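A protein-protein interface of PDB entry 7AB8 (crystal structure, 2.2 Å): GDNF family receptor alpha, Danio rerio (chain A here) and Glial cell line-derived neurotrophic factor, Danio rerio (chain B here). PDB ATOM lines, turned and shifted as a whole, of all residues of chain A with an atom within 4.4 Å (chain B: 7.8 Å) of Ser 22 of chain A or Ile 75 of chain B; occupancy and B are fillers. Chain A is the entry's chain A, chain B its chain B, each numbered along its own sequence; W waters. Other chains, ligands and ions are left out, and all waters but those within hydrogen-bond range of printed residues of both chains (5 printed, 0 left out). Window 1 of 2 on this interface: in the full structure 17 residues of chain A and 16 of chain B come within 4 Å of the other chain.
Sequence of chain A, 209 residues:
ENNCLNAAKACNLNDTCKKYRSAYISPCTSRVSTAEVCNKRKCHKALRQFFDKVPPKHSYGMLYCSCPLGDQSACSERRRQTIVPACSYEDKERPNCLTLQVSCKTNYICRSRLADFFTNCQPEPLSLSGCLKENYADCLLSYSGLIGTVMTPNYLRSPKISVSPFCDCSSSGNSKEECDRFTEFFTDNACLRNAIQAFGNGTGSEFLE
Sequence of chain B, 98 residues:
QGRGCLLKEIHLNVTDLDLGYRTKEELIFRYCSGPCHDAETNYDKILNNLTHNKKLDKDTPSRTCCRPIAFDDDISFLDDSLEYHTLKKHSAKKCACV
Water W2 lies within hydrogen-bond range of the side-chain carboxylate of Glu 25 of chain B (2.7 Å), the backbone NH of Glu 26 of chain B (3.0 Å) and the side-chain amide nitrogen of Asn 12 of chain A (3.2 Å). Water W4 lies within hydrogen-bond range of OG of Ser 26 of chain A (2.7 Å), O of Ser 22 of chain A (3.0 Å) and OD2 of Asp 74 of chain B (3.3 Å). Water W3 bridges the backbone carbonyl oxygen of Asn 12 of chain A (2.8 Å) and the backbone NH of Ile 28 of chain B (2.8 Å). Water W5 lies within hydrogen-bond range of OD1 of Asn 12 of chain A (2.9 Å), N of Ser 76 of chain B (2.9 Å) and O of Lys 18 of chain A (3.1 Å). Water W1 lies within hydrogen-bond range of the side-chain carboxylate (OD2) of Asp 73 of chain B (3.0 Å) and the side-chain amino group (NZ) of Lys 18 of chain A (3.2 Å).
The side-chain amino group (NZ) of Lys 18 of chain A sits at hydrogen-bond distance from the backbone carbonyl oxygen (O) of Asp 73 of chain B, 3.4 Å away. O of Glu 26 of chain B sits at hydrogen-bond distance from ND2 of Asn 12 of chain A (3.4 Å). The guanidinium group (NH1) of Arg 21 of chain A sits at hydrogen-bond distance from the backbone carbonyl oxygen (O) of Ser 76 of chain B (3.3 Å). OE2 of Glu 25 of chain B is in salt-bridge range of NH2 of Arg 21 of chain A (2.8 Å). The side-chain hydroxyl (OG) of Ser 22 of chain A lies within hydrogen-bond range of the side-chain hydroxyl (OG) of Ser 76 of chain B, at 2.7 Å. The side-chain carboxylate of Asp 72 of chain B is in salt-bridge range of the side-chain amino group of Lys 18 of chain A, at 3.0 Å. The side-chain carboxylate (OE1) of Glu 25 of chain B sits at hydrogen-bond distance from the side-chain amide nitrogen (ND2) of Asn 12 of chain A. The side-chain amide nitrogen (ND2) of Asn 12 of chain A lies within hydrogen-bond range of the backbone carbonyl oxygen (O) of Ser 76 of chain B, 3.0 Å away.
Ser 22 of chain A touches four residues of chain B. Of chain A, only Asn 12 (3.6 Å), Lys 18 (3.8 Å) and Ser 22 (3.4 Å) come within 4 Å of Ile 75 of chain B. Of the printed residues of chain B, Lys 19 of chain A touches Asp 73. Printed residues of chain A within 4 Å of Thr 86 of chain B: Ser 22 (3.6 Å), Ile 25 (3.8 Å) and Ser 26 (3.6 Å). Printed residues of chain A within 4 Å of Asp 74 of chain B: Lys 18 (3.6 Å) and Ser 22 (3.4 Å). Leu 27 of chain B touches none of the printed residues of chain A. Leu 17 of chain B touches none of the printed residues of chain A. The nearest printed residue of chain A that does not touch Ile 75 of chain B is Arg 21 of chain A (6.2 Å).
The backbone carbonyl oxygen of Ser 22 of chain A sits at hydrogen-bond distance from the side-chain hydroxyl of Ser 26 of chain A, 3.3 Å away. N of Val 14 of chain B lies within hydrogen-bond range of O of Glu 25 of chain B (2.9 Å). O of Ile 75 of chain B lies within hydrogen-bond range of N of Leu 87 of chain B (2.9 Å). OD1 of Asn 12 of chain A sits at hydrogen-bond distance from NH1 of Arg 21 of chain A (3.1 Å). The side-chain hydroxyl (OG1) of Thr 86 of chain B sits at hydrogen-bond distance from the side-chain hydroxyl (OG) of Ser 76 of chain B, at 2.7 Å. N of Asp 72 of chain B sits at hydrogen-bond distance from O of Ser 91 of chain B.
Asn 12 of chain A touches Ile 75 of chain B (ND2 to CD1, 3.6 Å). Lys 18 of chain A touches Asp 74 of chain B. Lys 18 of chain A touches Ile 75 of chain B. Asp 73 of chain B touches Lys 19 of chain A. Ser 22 of chain A touches Asp 74 of chain B (CB to O, 3.4 Å). Ile 75 of chain B touches Ser 22 of chain A (C to OG, 3.4 Å). Ser 22 of chain A touches Thr 86 of chain B. CG2 of Ile 25 of chain A touches OG of Ser 76 of chain B (3.4 Å). Ile 25 of chain A touches Thr 86 of chain B (CG2 to OG1, 3.8 Å). CG2 of Thr 86 of chain B touches OG of Ser 26 of chain A (3.6 Å).
Among the printed residues, 18 pairs touch across the chains. Among the printed residues, Asp or Glu carboxylates within 4 Å of a Lys or Arg side-chain nitrogen of the other chain: Lys 18 of chain A with Asp 72 of chain B and Arg 21 of chain A with Glu 25 of chain B.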
ATOM      1  N   ASN A  12      15.572 -34.133 -16.561  1.00  0.00           N
ATOM      2  CA  ASN A  12      15.807 -32.709 -16.770  1.00  0.00           C
ATOM      3  C   ASN A  12      15.172 -31.851 -15.683  1.00  0.00           C
ATOM      4  O   ASN A  12      15.576 -30.696 -15.509  1.00  0.00           O
ATOM      5  CB  ASN A  12      15.287 -32.286 -18.145  1.00  0.00           C
ATOM      6  CG  ASN A  12      16.321 -32.473 -19.242  1.00  0.00           C
ATOM      7  OD1 ASN A  12      17.411 -32.992 -19.001  1.00  0.00           O
ATOM      8  ND2 ASN A  12      15.983 -32.048 -20.453  1.00  0.00           N
ATOM      9  N   LYS A  18      19.975 -33.729 -14.574  1.00  0.00           N
ATOM     10  CA  LYS A  18      20.080 -32.798 -15.694  1.00  0.00           C
ATOM     11  C   LYS A  18      21.530 -32.407 -15.949  1.00  0.00           C
ATOM     12  O   LYS A  18      21.987 -32.383 -17.097  1.00  0.00           O
ATOM     13  CB  LYS A  18      19.231 -31.555 -15.425  1.00  0.00           C
ATOM     14  CG  LYS A  18      19.095 -30.619 -16.615  1.00  0.00           C
ATOM     15  CD  LYS A  18      18.896 -29.178 -16.166  1.00  0.00           C
ATOM     16  CE  LYS A  18      20.226 -28.480 -15.928  1.00  0.00           C
ATOM     17  NZ  LYS A  18      20.048 -27.130 -15.324  1.00  0.00           N
ATOM     18  N   LYS A  19      22.271 -32.103 -14.881  1.00  0.00           N
ATOM     19  CA  LYS A  19      23.650 -31.650 -15.030  1.00  0.00           C
ATOM     20  C   LYS A  19      24.523 -32.726 -15.663  1.00  0.00           C
ATOM     21  O   LYS A  19      25.227 -32.474 -16.648  1.00  0.00           O
ATOM     22  CB  LYS A  19      24.212 -31.234 -13.670  1.00  0.00           C
ATOM     23  CG  LYS A  19      25.729 -31.136 -13.629  1.00  0.00           C
ATOM     24  CD  LYS A  19      26.218 -30.688 -12.261  1.00  0.00           C
ATOM     25  CE  LYS A  19      27.735 -30.575 -12.226  1.00  0.00           C
ATOM     26  NZ  LYS A  19      28.211 -29.834 -11.025  1.00  0.00           N
ATOM     27  N   TYR A  20      24.487 -33.941 -15.113  1.00  0.00           N
ATOM     28  CA  TYR A  20      25.383 -34.990 -15.579  1.00  0.00           C
ATOM     29  C   TYR A  20      24.914 -35.641 -16.873  1.00  0.00           C
ATOM     30  O   TYR A  20      25.737 -36.220 -17.590  1.00  0.00           O
ATOM     31  CB  TYR A  20      25.563 -36.041 -14.483  1.00  0.00           C
ATOM     32  CG  TYR A  20      26.370 -35.508 -13.324  1.00  0.00           C
ATOM     33  CD1 TYR A  20      27.716 -35.203 -13.478  1.00  0.00           C
ATOM     34  CD2 TYR A  20      25.783 -35.278 -12.087  1.00  0.00           C
ATOM     35  CE1 TYR A  20      28.460 -34.701 -12.430  1.00  0.00           C
ATOM     36  CE2 TYR A  20      26.520 -34.776 -11.031  1.00  0.00           C
ATOM     37  CZ  TYR A  20      27.857 -34.490 -11.208  1.00  0.00           C
ATOM     38  OH  TYR A  20      28.595 -33.988 -10.161  1.00  0.00           O
ATOM     39  N   ARG A  21      23.621 -35.556 -17.194  1.00  0.00           N
ATOM     40  CA  ARG A  21      23.168 -35.989 -18.511  1.00  0.00           C
ATOM     41  C   ARG A  21      23.747 -35.094 -19.599  1.00  0.00           C
ATOM     42  O   ARG A  21      24.299 -35.583 -20.592  1.00  0.00           O
ATOM     43  CB  ARG A  21      21.641 -35.990 -18.571  1.00  0.00           C
ATOM     44  CG  ARG A  21      21.074 -36.518 -19.874  1.00  0.00           C
ATOM     45  CD  ARG A  21      19.695 -35.943 -20.139  1.00  0.00           C
ATOM     46  NE  ARG A  21      19.048 -36.582 -21.280  1.00  0.00           N
ATOM     47  CZ  ARG A  21      17.908 -36.166 -21.820  1.00  0.00           C
ATOM     48  NH1 ARG A  21      17.284 -35.107 -21.323  1.00  0.00           N
ATOM     49  NH2 ARG A  21      17.391 -36.810 -22.857  1.00  0.00           N
ATOM     50  N   SER A  22      23.634 -33.775 -19.422  1.00  0.00           N
ATOM     51  CA  SER A  22      24.254 -32.847 -20.361  1.00  0.00           C
ATOM     52  C   SER A  22      25.771 -32.961 -20.333  1.00  0.00           C
ATOM     53  O   SER A  22      26.433 -32.700 -21.345  1.00  0.00           O
ATOM     54  CB  SER A  22      23.825 -31.415 -20.043  1.00  0.00           C
ATOM     55  OG  SER A  22      23.873 -30.597 -21.198  1.00  0.00           O
ATOM     56  N   ALA A  23      26.338 -33.359 -19.191  1.00  0.00           N
ATOM     57  CA  ALA A  23      27.786 -33.467 -19.068  1.00  0.00           C
ATOM     58  C   ALA A  23      28.365 -34.587 -19.922  1.00  0.00           C
ATOM     59  O   ALA A  23      29.569 -34.575 -20.196  1.00  0.00           O
ATOM     60  CB  ALA A  23      28.179 -33.674 -17.606  1.00  0.00           C
ATOM     61  N   TYR A  24      27.551 -35.557 -20.341  1.00  0.00           N
ATOM     62  CA  TYR A  24      28.024 -36.568 -21.278  1.00  0.00           C
ATOM     63  C   TYR A  24      27.490 -36.386 -22.687  1.00  0.00           C
ATOM     64  O   TYR A  24      28.152 -36.799 -23.638  1.00  0.00           O
ATOM     65  CB  TYR A  24      27.700 -37.984 -20.767  1.00  0.00           C
ATOM     66  CG  TYR A  24      26.288 -38.513 -20.962  1.00  0.00           C
ATOM     67  CD1 TYR A  24      25.861 -39.004 -22.193  1.00  0.00           C
ATOM     68  CD2 TYR A  24      25.402 -38.582 -19.892  1.00  0.00           C
ATOM     69  CE1 TYR A  24      24.582 -39.508 -22.361  1.00  0.00           C
ATOM     70  CE2 TYR A  24      24.123 -39.086 -20.050  1.00  0.00           C
ATOM     71  CZ  TYR A  24      23.718 -39.547 -21.286  1.00  0.00           C
ATOM     72  OH  TYR A  24      22.446 -40.049 -21.446  1.00  0.00           O
ATOM     73  N   ILE A  25      26.325 -35.756 -22.851  1.00  0.00           N
ATOM     74  CA  ILE A  25      25.815 -35.510 -24.194  1.00  0.00           C
ATOM     75  C   ILE A  25      26.712 -34.527 -24.943  1.00  0.00           C
ATOM     76  O   ILE A  25      26.894 -34.648 -26.162  1.00  0.00           O
ATOM     77  CB  ILE A  25      24.352 -35.033 -24.120  1.00  0.00           C
ATOM     78  CG1 ILE A  25      23.437 -36.227 -23.842  1.00  0.00           C
ATOM     79  CG2 ILE A  25      23.934 -34.330 -25.404  1.00  0.00           C
ATOM     80  CD1 ILE A  25      22.056 -35.855 -23.367  1.00  0.00           C
ATOM     81  N   SER A  26      27.317 -33.563 -24.231  1.00  0.00           N
ATOM     82  CA  SER A  26      28.185 -32.597 -24.908  1.00  0.00           C
ATOM     83  C   SER A  26      29.438 -33.255 -25.473  1.00  0.00           C
ATOM     84  O   SER A  26      29.691 -33.126 -26.684  1.00  0.00           O
ATOM     85  CB  SER A  26      28.510 -31.432 -23.968  1.00  0.00           C
ATOM     86  OG  SER A  26      27.367 -30.632 -23.728  1.00  0.00           O
ATOM     87  N   VAL B  14      10.112 -27.678 -23.766  1.00  0.00           N
ATOM     88  CA  VAL B  14      11.179 -27.083 -24.566  1.00  0.00           C
ATOM     89  C   VAL B  14      10.591 -26.280 -25.721  1.00  0.00           C
ATOM     90  O   VAL B  14      11.142 -25.242 -26.112  1.00  0.00           O
ATOM     91  CB  VAL B  14      12.153 -28.173 -25.062  1.00  0.00           C
ATOM     92  CG1 VAL B  14      13.101 -27.615 -26.116  1.00  0.00           C
ATOM     93  CG2 VAL B  14      12.945 -28.743 -23.895  1.00  0.00           C
ATOM     94  N   LEU B  17       9.959 -22.481 -25.487  1.00  0.00           N
ATOM     95  CA  LEU B  17      11.039 -21.523 -25.685  1.00  0.00           C
ATOM     96  C   LEU B  17      11.016 -20.903 -27.076  1.00  0.00           C
ATOM     97  O   LEU B  17      11.650 -19.863 -27.284  1.00  0.00           O
ATOM     98  CB  LEU B  17      12.389 -22.199 -25.437  1.00  0.00           C
ATOM     99  CG  LEU B  17      12.537 -22.914 -24.091  1.00  0.00           C
ATOM    100  CD1 LEU B  17      13.878 -23.625 -24.001  1.00  0.00           C
ATOM    101  CD2 LEU B  17      12.365 -21.936 -22.942  1.00  0.00           C
ATOM    102  N   GLU B  25      10.527 -32.899 -24.761  1.00  0.00           N
ATOM    103  CA  GLU B  25      11.247 -32.786 -23.504  1.00  0.00           C
ATOM    104  C   GLU B  25      10.878 -31.486 -22.792  1.00  0.00           C
ATOM    105  O   GLU B  25      10.344 -30.547 -23.390  1.00  0.00           O
ATOM    106  CB  GLU B  25      12.756 -32.859 -23.744  1.00  0.00           C
ATOM    107  CG  GLU B  25      13.233 -34.224 -24.224  1.00  0.00           C
ATOM    108  CD  GLU B  25      14.550 -34.642 -23.595  1.00  0.00           C
ATOM    109  OE1 GLU B  25      14.883 -34.124 -22.508  1.00  0.00           O
ATOM    110  OE2 GLU B  25      15.253 -35.486 -24.190  1.00  0.00           O
ATOM    111  N   GLU B  26      11.165 -31.446 -21.493  1.00  0.00           N
ATOM    112  CA  GLU B  26      10.792 -30.330 -20.635  1.00  0.00           C
ATOM    113  C   GLU B  26      12.028 -29.798 -19.918  1.00  0.00           C
ATOM    114  O   GLU B  26      13.126 -30.352 -20.023  1.00  0.00           O
ATOM    115  CB  GLU B  26       9.715 -30.742 -19.624  1.00  0.00           C
ATOM    116  CG  GLU B  26       8.393 -31.133 -20.253  1.00  0.00           C
ATOM    117  CD  GLU B  26       7.412 -31.688 -19.239  1.00  0.00           C
ATOM    118  OE1 GLU B  26       7.775 -31.779 -18.048  1.00  0.00           O
ATOM    119  OE2 GLU B  26       6.290 -32.065 -19.641  1.00  0.00           O
ATOM    120  N   LEU B  27      11.835 -28.712 -19.171  1.00  0.00           N
ATOM    121  CA  LEU B  27      12.931 -28.076 -18.457  1.00  0.00           C
ATOM    122  C   LEU B  27      12.369 -27.157 -17.384  1.00  0.00           C
ATOM    123  O   LEU B  27      11.186 -26.805 -17.394  1.00  0.00           O
ATOM    124  CB  LEU B  27      13.834 -27.282 -19.407  1.00  0.00           C
ATOM    125  CG  LEU B  27      13.323 -25.919 -19.877  1.00  0.00           C
ATOM    126  CD1 LEU B  27      14.484 -24.963 -20.099  1.00  0.00           C
ATOM    127  CD2 LEU B  27      12.498 -26.065 -21.145  1.00  0.00           C
ATOM    128  N   ILE B  28      13.240 -26.779 -16.455  1.00  0.00           N
ATOM    129  CA  ILE B  28      12.958 -25.749 -15.464  1.00  0.00           C
ATOM    130  C   ILE B  28      13.751 -24.516 -15.874  1.00  0.00           C
ATOM    131  O   ILE B  28      14.987 -24.512 -15.805  1.00  0.00           O
ATOM    132  CB  ILE B  28      13.324 -26.196 -14.043  1.00  0.00           C
ATOM    133  CG1 ILE B  28      12.505 -27.420 -13.632  1.00  0.00           C
ATOM    134  CG2 ILE B  28      13.116 -25.054 -13.057  1.00  0.00           C
ATOM    135  CD1 ILE B  28      11.013 -27.233 -13.772  1.00  0.00           C
ATOM    136  N   PHE B  29      13.051 -23.476 -16.315  1.00  0.00           N
ATOM    137  CA  PHE B  29      13.690 -22.220 -16.680  1.00  0.00           C
ATOM    138  C   PHE B  29      13.695 -21.287 -15.477  1.00  0.00           C
ATOM    139  O   PHE B  29      12.648 -21.043 -14.870  1.00  0.00           O
ATOM    140  CB  PHE B  29      12.970 -21.563 -17.858  1.00  0.00           C
ATOM    141  CG  PHE B  29      13.466 -20.181 -18.175  1.00  0.00           C
ATOM    142  CD1 PHE B  29      14.738 -19.988 -18.688  1.00  0.00           C
ATOM    143  CD2 PHE B  29      12.663 -19.075 -17.957  1.00  0.00           C
ATOM    144  CE1 PHE B  29      15.198 -18.718 -18.979  1.00  0.00           C
ATOM    145  CE2 PHE B  29      13.118 -17.801 -18.246  1.00  0.00           C
ATOM    146  CZ  PHE B  29      14.387 -17.623 -18.758  1.00  0.00           C
ATOM    147  N   ASP B  72      22.868 -21.254 -14.882  1.00  0.00           N
ATOM    148  CA  ASP B  72      22.667 -22.640 -14.498  1.00  0.00           C
ATOM    149  C   ASP B  72      23.498 -23.570 -15.383  1.00  0.00           C
ATOM    150  O   ASP B  72      24.092 -23.158 -16.384  1.00  0.00           O
ATOM    151  CB  ASP B  72      21.181 -22.997 -14.589  1.00  0.00           C
ATOM    152  CG  ASP B  72      20.814 -24.210 -13.759  1.00  0.00           C
ATOM    153  OD1 ASP B  72      21.705 -24.762 -13.080  1.00  0.00           O
ATOM    154  OD2 ASP B  72      19.631 -24.611 -13.787  1.00  0.00           O
ATOM    155  N   ASP B  73      23.536 -24.843 -14.995  1.00  0.00           N
ATOM    156  CA  ASP B  73      24.226 -25.847 -15.794  1.00  0.00           C
ATOM    157  C   ASP B  73      23.575 -25.978 -17.166  1.00  0.00           C
ATOM    158  O   ASP B  73      22.395 -25.669 -17.352  1.00  0.00           O
ATOM    159  CB  ASP B  73      24.209 -27.202 -15.084  1.00  0.00           C
ATOM    160  CG  ASP B  73      24.922 -27.174 -13.748  1.00  0.00           C
ATOM    161  OD1 ASP B  73      26.128 -26.847 -13.722  1.00  0.00           O
ATOM    162  OD2 ASP B  73      24.279 -27.487 -12.724  1.00  0.00           O
ATOM    163  N   ASP B  74      24.362 -26.440 -18.135  1.00  0.00           N
ATOM    164  CA  ASP B  74      23.829 -26.717 -19.460  1.00  0.00           C
ATOM    165  C   ASP B  74      22.723 -27.762 -19.377  1.00  0.00           C
ATOM    166  O   ASP B  74      22.712 -28.621 -18.491  1.00  0.00           O
ATOM    167  CB  ASP B  74      24.933 -27.216 -20.394  1.00  0.00           C
ATOM    168  CG  ASP B  74      26.016 -26.184 -20.626  1.00  0.00           C
ATOM    169  OD1 ASP B  74      25.883 -25.051 -20.119  1.00  0.00           O
ATOM    170  OD2 ASP B  74      27.004 -26.511 -21.315  1.00  0.00           O
ATOM    171  N   ILE B  75      21.782 -27.684 -20.313  1.00  0.00           N
ATOM    172  CA  ILE B  75      20.712 -28.665 -20.431  1.00  0.00           C
ATOM    173  C   ILE B  75      20.781 -29.296 -21.813  1.00  0.00           C
ATOM    174  O   ILE B  75      21.132 -28.630 -22.794  1.00  0.00           O
ATOM    175  CB  ILE B  75      19.322 -28.043 -20.175  1.00  0.00           C
ATOM    176  CG1 ILE B  75      18.253 -29.138 -20.164  1.00  0.00           C
ATOM    177  CG2 ILE B  75      18.998 -26.982 -21.219  1.00  0.00           C
ATOM    178  CD1 ILE B  75      16.989 -28.751 -19.462  1.00  0.00           C
ATOM    179  N   SER B  76      20.463 -30.584 -21.881  1.00  0.00           N
ATOM    180  CA  SER B  76      20.438 -31.327 -23.128  1.00  0.00           C
ATOM    181  C   SER B  76      19.071 -31.973 -23.314  1.00  0.00           C
ATOM    182  O   SER B  76      18.314 -32.159 -22.357  1.00  0.00           O
ATOM    183  CB  SER B  76      21.532 -32.400 -23.153  1.00  0.00           C
ATOM    184  OG  SER B  76      22.811 -31.822 -23.337  1.00  0.00           O
ATOM    185  N   PHE B  77      18.760 -32.310 -24.563  1.00  0.00           N
ATOM    186  CA  PHE B  77      17.510 -32.987 -24.876  1.00  0.00           C
ATOM    187  C   PHE B  77      17.616 -33.620 -26.255  1.00  0.00           C
ATOM    188  O   PHE B  77      18.443 -33.224 -27.080  1.00  0.00           O
ATOM    189  CB  PHE B  77      16.310 -32.030 -24.806  1.00  0.00           C
ATOM    190  CG  PHE B  77      16.463 -30.791 -25.643  1.00  0.00           C
ATOM    191  CD1 PHE B  77      16.122 -30.798 -26.985  1.00  0.00           C
ATOM    192  CD2 PHE B  77      16.933 -29.615 -25.082  1.00  0.00           C
ATOM    193  CE1 PHE B  77      16.257 -29.659 -27.756  1.00  0.00           C
ATOM    194  CE2 PHE B  77      17.071 -28.472 -25.847  1.00  0.00           C
ATOM    195  CZ  PHE B  77      16.732 -28.495 -27.187  1.00  0.00           C
ATOM    196  N   HIS B  85      20.584 -31.995 -28.659  1.00  0.00           N
ATOM    197  CA  HIS B  85      20.916 -30.579 -28.628  1.00  0.00           C
ATOM    198  C   HIS B  85      21.278 -30.185 -27.204  1.00  0.00           C
ATOM    199  O   HIS B  85      20.746 -30.737 -26.238  1.00  0.00           O
ATOM    200  CB  HIS B  85      19.756 -29.704 -29.125  1.00  0.00           C
ATOM    201  CG  HIS B  85      19.238 -30.089 -30.476  1.00  0.00           C
ATOM    202  ND1 HIS B  85      19.734 -29.550 -31.644  1.00  0.00           N
ATOM    203  CD2 HIS B  85      18.265 -30.955 -30.845  1.00  0.00           C
ATOM    204  CE1 HIS B  85      19.090 -30.069 -32.674  1.00  0.00           C
ATOM    205  NE2 HIS B  85      18.193 -30.924 -32.217  1.00  0.00           N
ATOM    206  N   THR B  86      22.189 -29.224 -27.082  1.00  0.00           N
ATOM    207  CA  THR B  86      22.621 -28.715 -25.787  1.00  0.00           C
ATOM    208  C   THR B  86      22.513 -27.199 -25.789  1.00  0.00           C
ATOM    209  O   THR B  86      23.000 -26.540 -26.714  1.00  0.00           O
ATOM    210  CB  THR B  86      24.058 -29.142 -25.466  1.00  0.00           C
ATOM    211  OG1 THR B  86      24.130 -30.572 -25.388  1.00  0.00           O
ATOM    212  CG2 THR B  86      24.509 -28.545 -24.141  1.00  0.00           C
ATOM    213  N   LEU B  87      21.872 -26.650 -24.761  1.00  0.00           N
ATOM    214  CA  LEU B  87      21.724 -25.211 -24.596  1.00  0.00           C
ATOM    215  C   LEU B  87      22.603 -24.743 -23.445  1.00  0.00           C
ATOM    216  O   LEU B  87      22.589 -25.342 -22.365  1.00  0.00           O
ATOM    217  CB  LEU B  87      20.263 -24.835 -24.334  1.00  0.00           C
ATOM    218  CG  LEU B  87      19.278 -25.121 -25.469  1.00  0.00           C
ATOM    219  CD1 LEU B  87      17.903 -24.571 -25.130  1.00  0.00           C
ATOM    220  CD2 LEU B  87      19.787 -24.534 -26.776  1.00  0.00           C
ATOM    221  N   LYS B  88      23.362 -23.676 -23.678  1.00  0.00           N
ATOM    222  CA  LYS B  88      24.256 -23.112 -22.679  1.00  0.00           C
ATOM    223  C   LYS B  88      23.819 -21.695 -22.335  1.00  0.00           C
ATOM    224  O   LYS B  88      23.304 -20.965 -23.188  1.00  0.00           O
ATOM    225  CB  LYS B  88      25.707 -23.103 -23.174  1.00  0.00           C
ATOM    226  CG  LYS B  88      26.154 -24.412 -23.798  1.00  0.00           C
ATOM    227  CD  LYS B  88      27.636 -24.389 -24.127  1.00  0.00           C
ATOM    228  CE  LYS B  88      28.115 -25.750 -24.601  1.00  0.00           C
ATOM    229  NZ  LYS B  88      29.598 -25.862 -24.549  1.00  0.00           N
ATOM    230  N   LYS B  89      24.036 -21.316 -21.075  1.00  0.00           N
ATOM    231  CA  LYS B  89      23.651 -19.999 -20.566  1.00  0.00           C
ATOM    232  C   LYS B  89      22.187 -19.702 -20.883  1.00  0.00           C
ATOM    233  O   LYS B  89      21.828 -18.627 -21.371  1.00  0.00           O
ATOM    234  CB  LYS B  89      24.571 -18.908 -21.114  1.00  0.00           C
ATOM    235  CG  LYS B  89      26.044 -19.143 -20.823  1.00  0.00           C
ATOM    236  CD  LYS B  89      26.732 -17.861 -20.385  1.00  0.00           C
ATOM    237  CE  LYS B  89      28.212 -18.088 -20.124  1.00  0.00           C
ATOM    238  NZ  LYS B  89      29.006 -16.847 -20.332  1.00  0.00           N
ATOM    239  N   HIS B  90      21.334 -20.688 -20.607  1.00  0.00           N
ATOM    240  CA  HIS B  90      19.910 -20.599 -20.894  1.00  0.00           C
ATOM    241  C   HIS B  90      19.073 -20.243 -19.675  1.00  0.00           C
ATOM    242  O   HIS B  90      17.939 -19.782 -19.837  1.00  0.00           O
ATOM    243  CB  HIS B  90      19.403 -21.929 -21.457  1.00  0.00           C
ATOM    244  CG  HIS B  90      19.287 -23.006 -20.423  1.00  0.00           C
ATOM    245  ND1 HIS B  90      20.387 -23.573 -19.815  1.00  0.00           N
ATOM    246  CD2 HIS B  90      18.204 -23.606 -19.876  1.00  0.00           C
ATOM    247  CE1 HIS B  90      19.987 -24.482 -18.945  1.00  0.00           C
ATOM    248  NE2 HIS B  90      18.667 -24.522 -18.961  1.00  0.00           N
ATOM    249  N   SER B  91      19.598 -20.456 -18.472  1.00  0.00           N
ATOM    250  CA  SER B  91      18.838 -20.289 -17.245  1.00  0.00           C
ATOM    251  C   SER B  91      19.719 -19.633 -16.194  1.00  0.00           C
ATOM    252  O   SER B  91      20.921 -19.905 -16.123  1.00  0.00           O
ATOM    253  CB  SER B  91      18.316 -21.637 -16.733  1.00  0.00           C
ATOM    254  OG  SER B  91      17.355 -21.462 -15.708  1.00  0.00           O
HETATM  255  O   HOH W   1      21.499 -28.669 -12.967  1.00  0.00           O
HETATM  256  O   HOH W   2      13.111 -33.525 -20.605  1.00  0.00           O
HETATM  257  O   HOH W   3      15.750 -27.997 -16.026  1.00  0.00           O
HETATM  258  O   HOH W   4      26.798 -29.763 -21.239  1.00  0.00           O
HETATM  259  O   HOH W   5      20.185 -32.342 -19.577  1.00  0.00           O
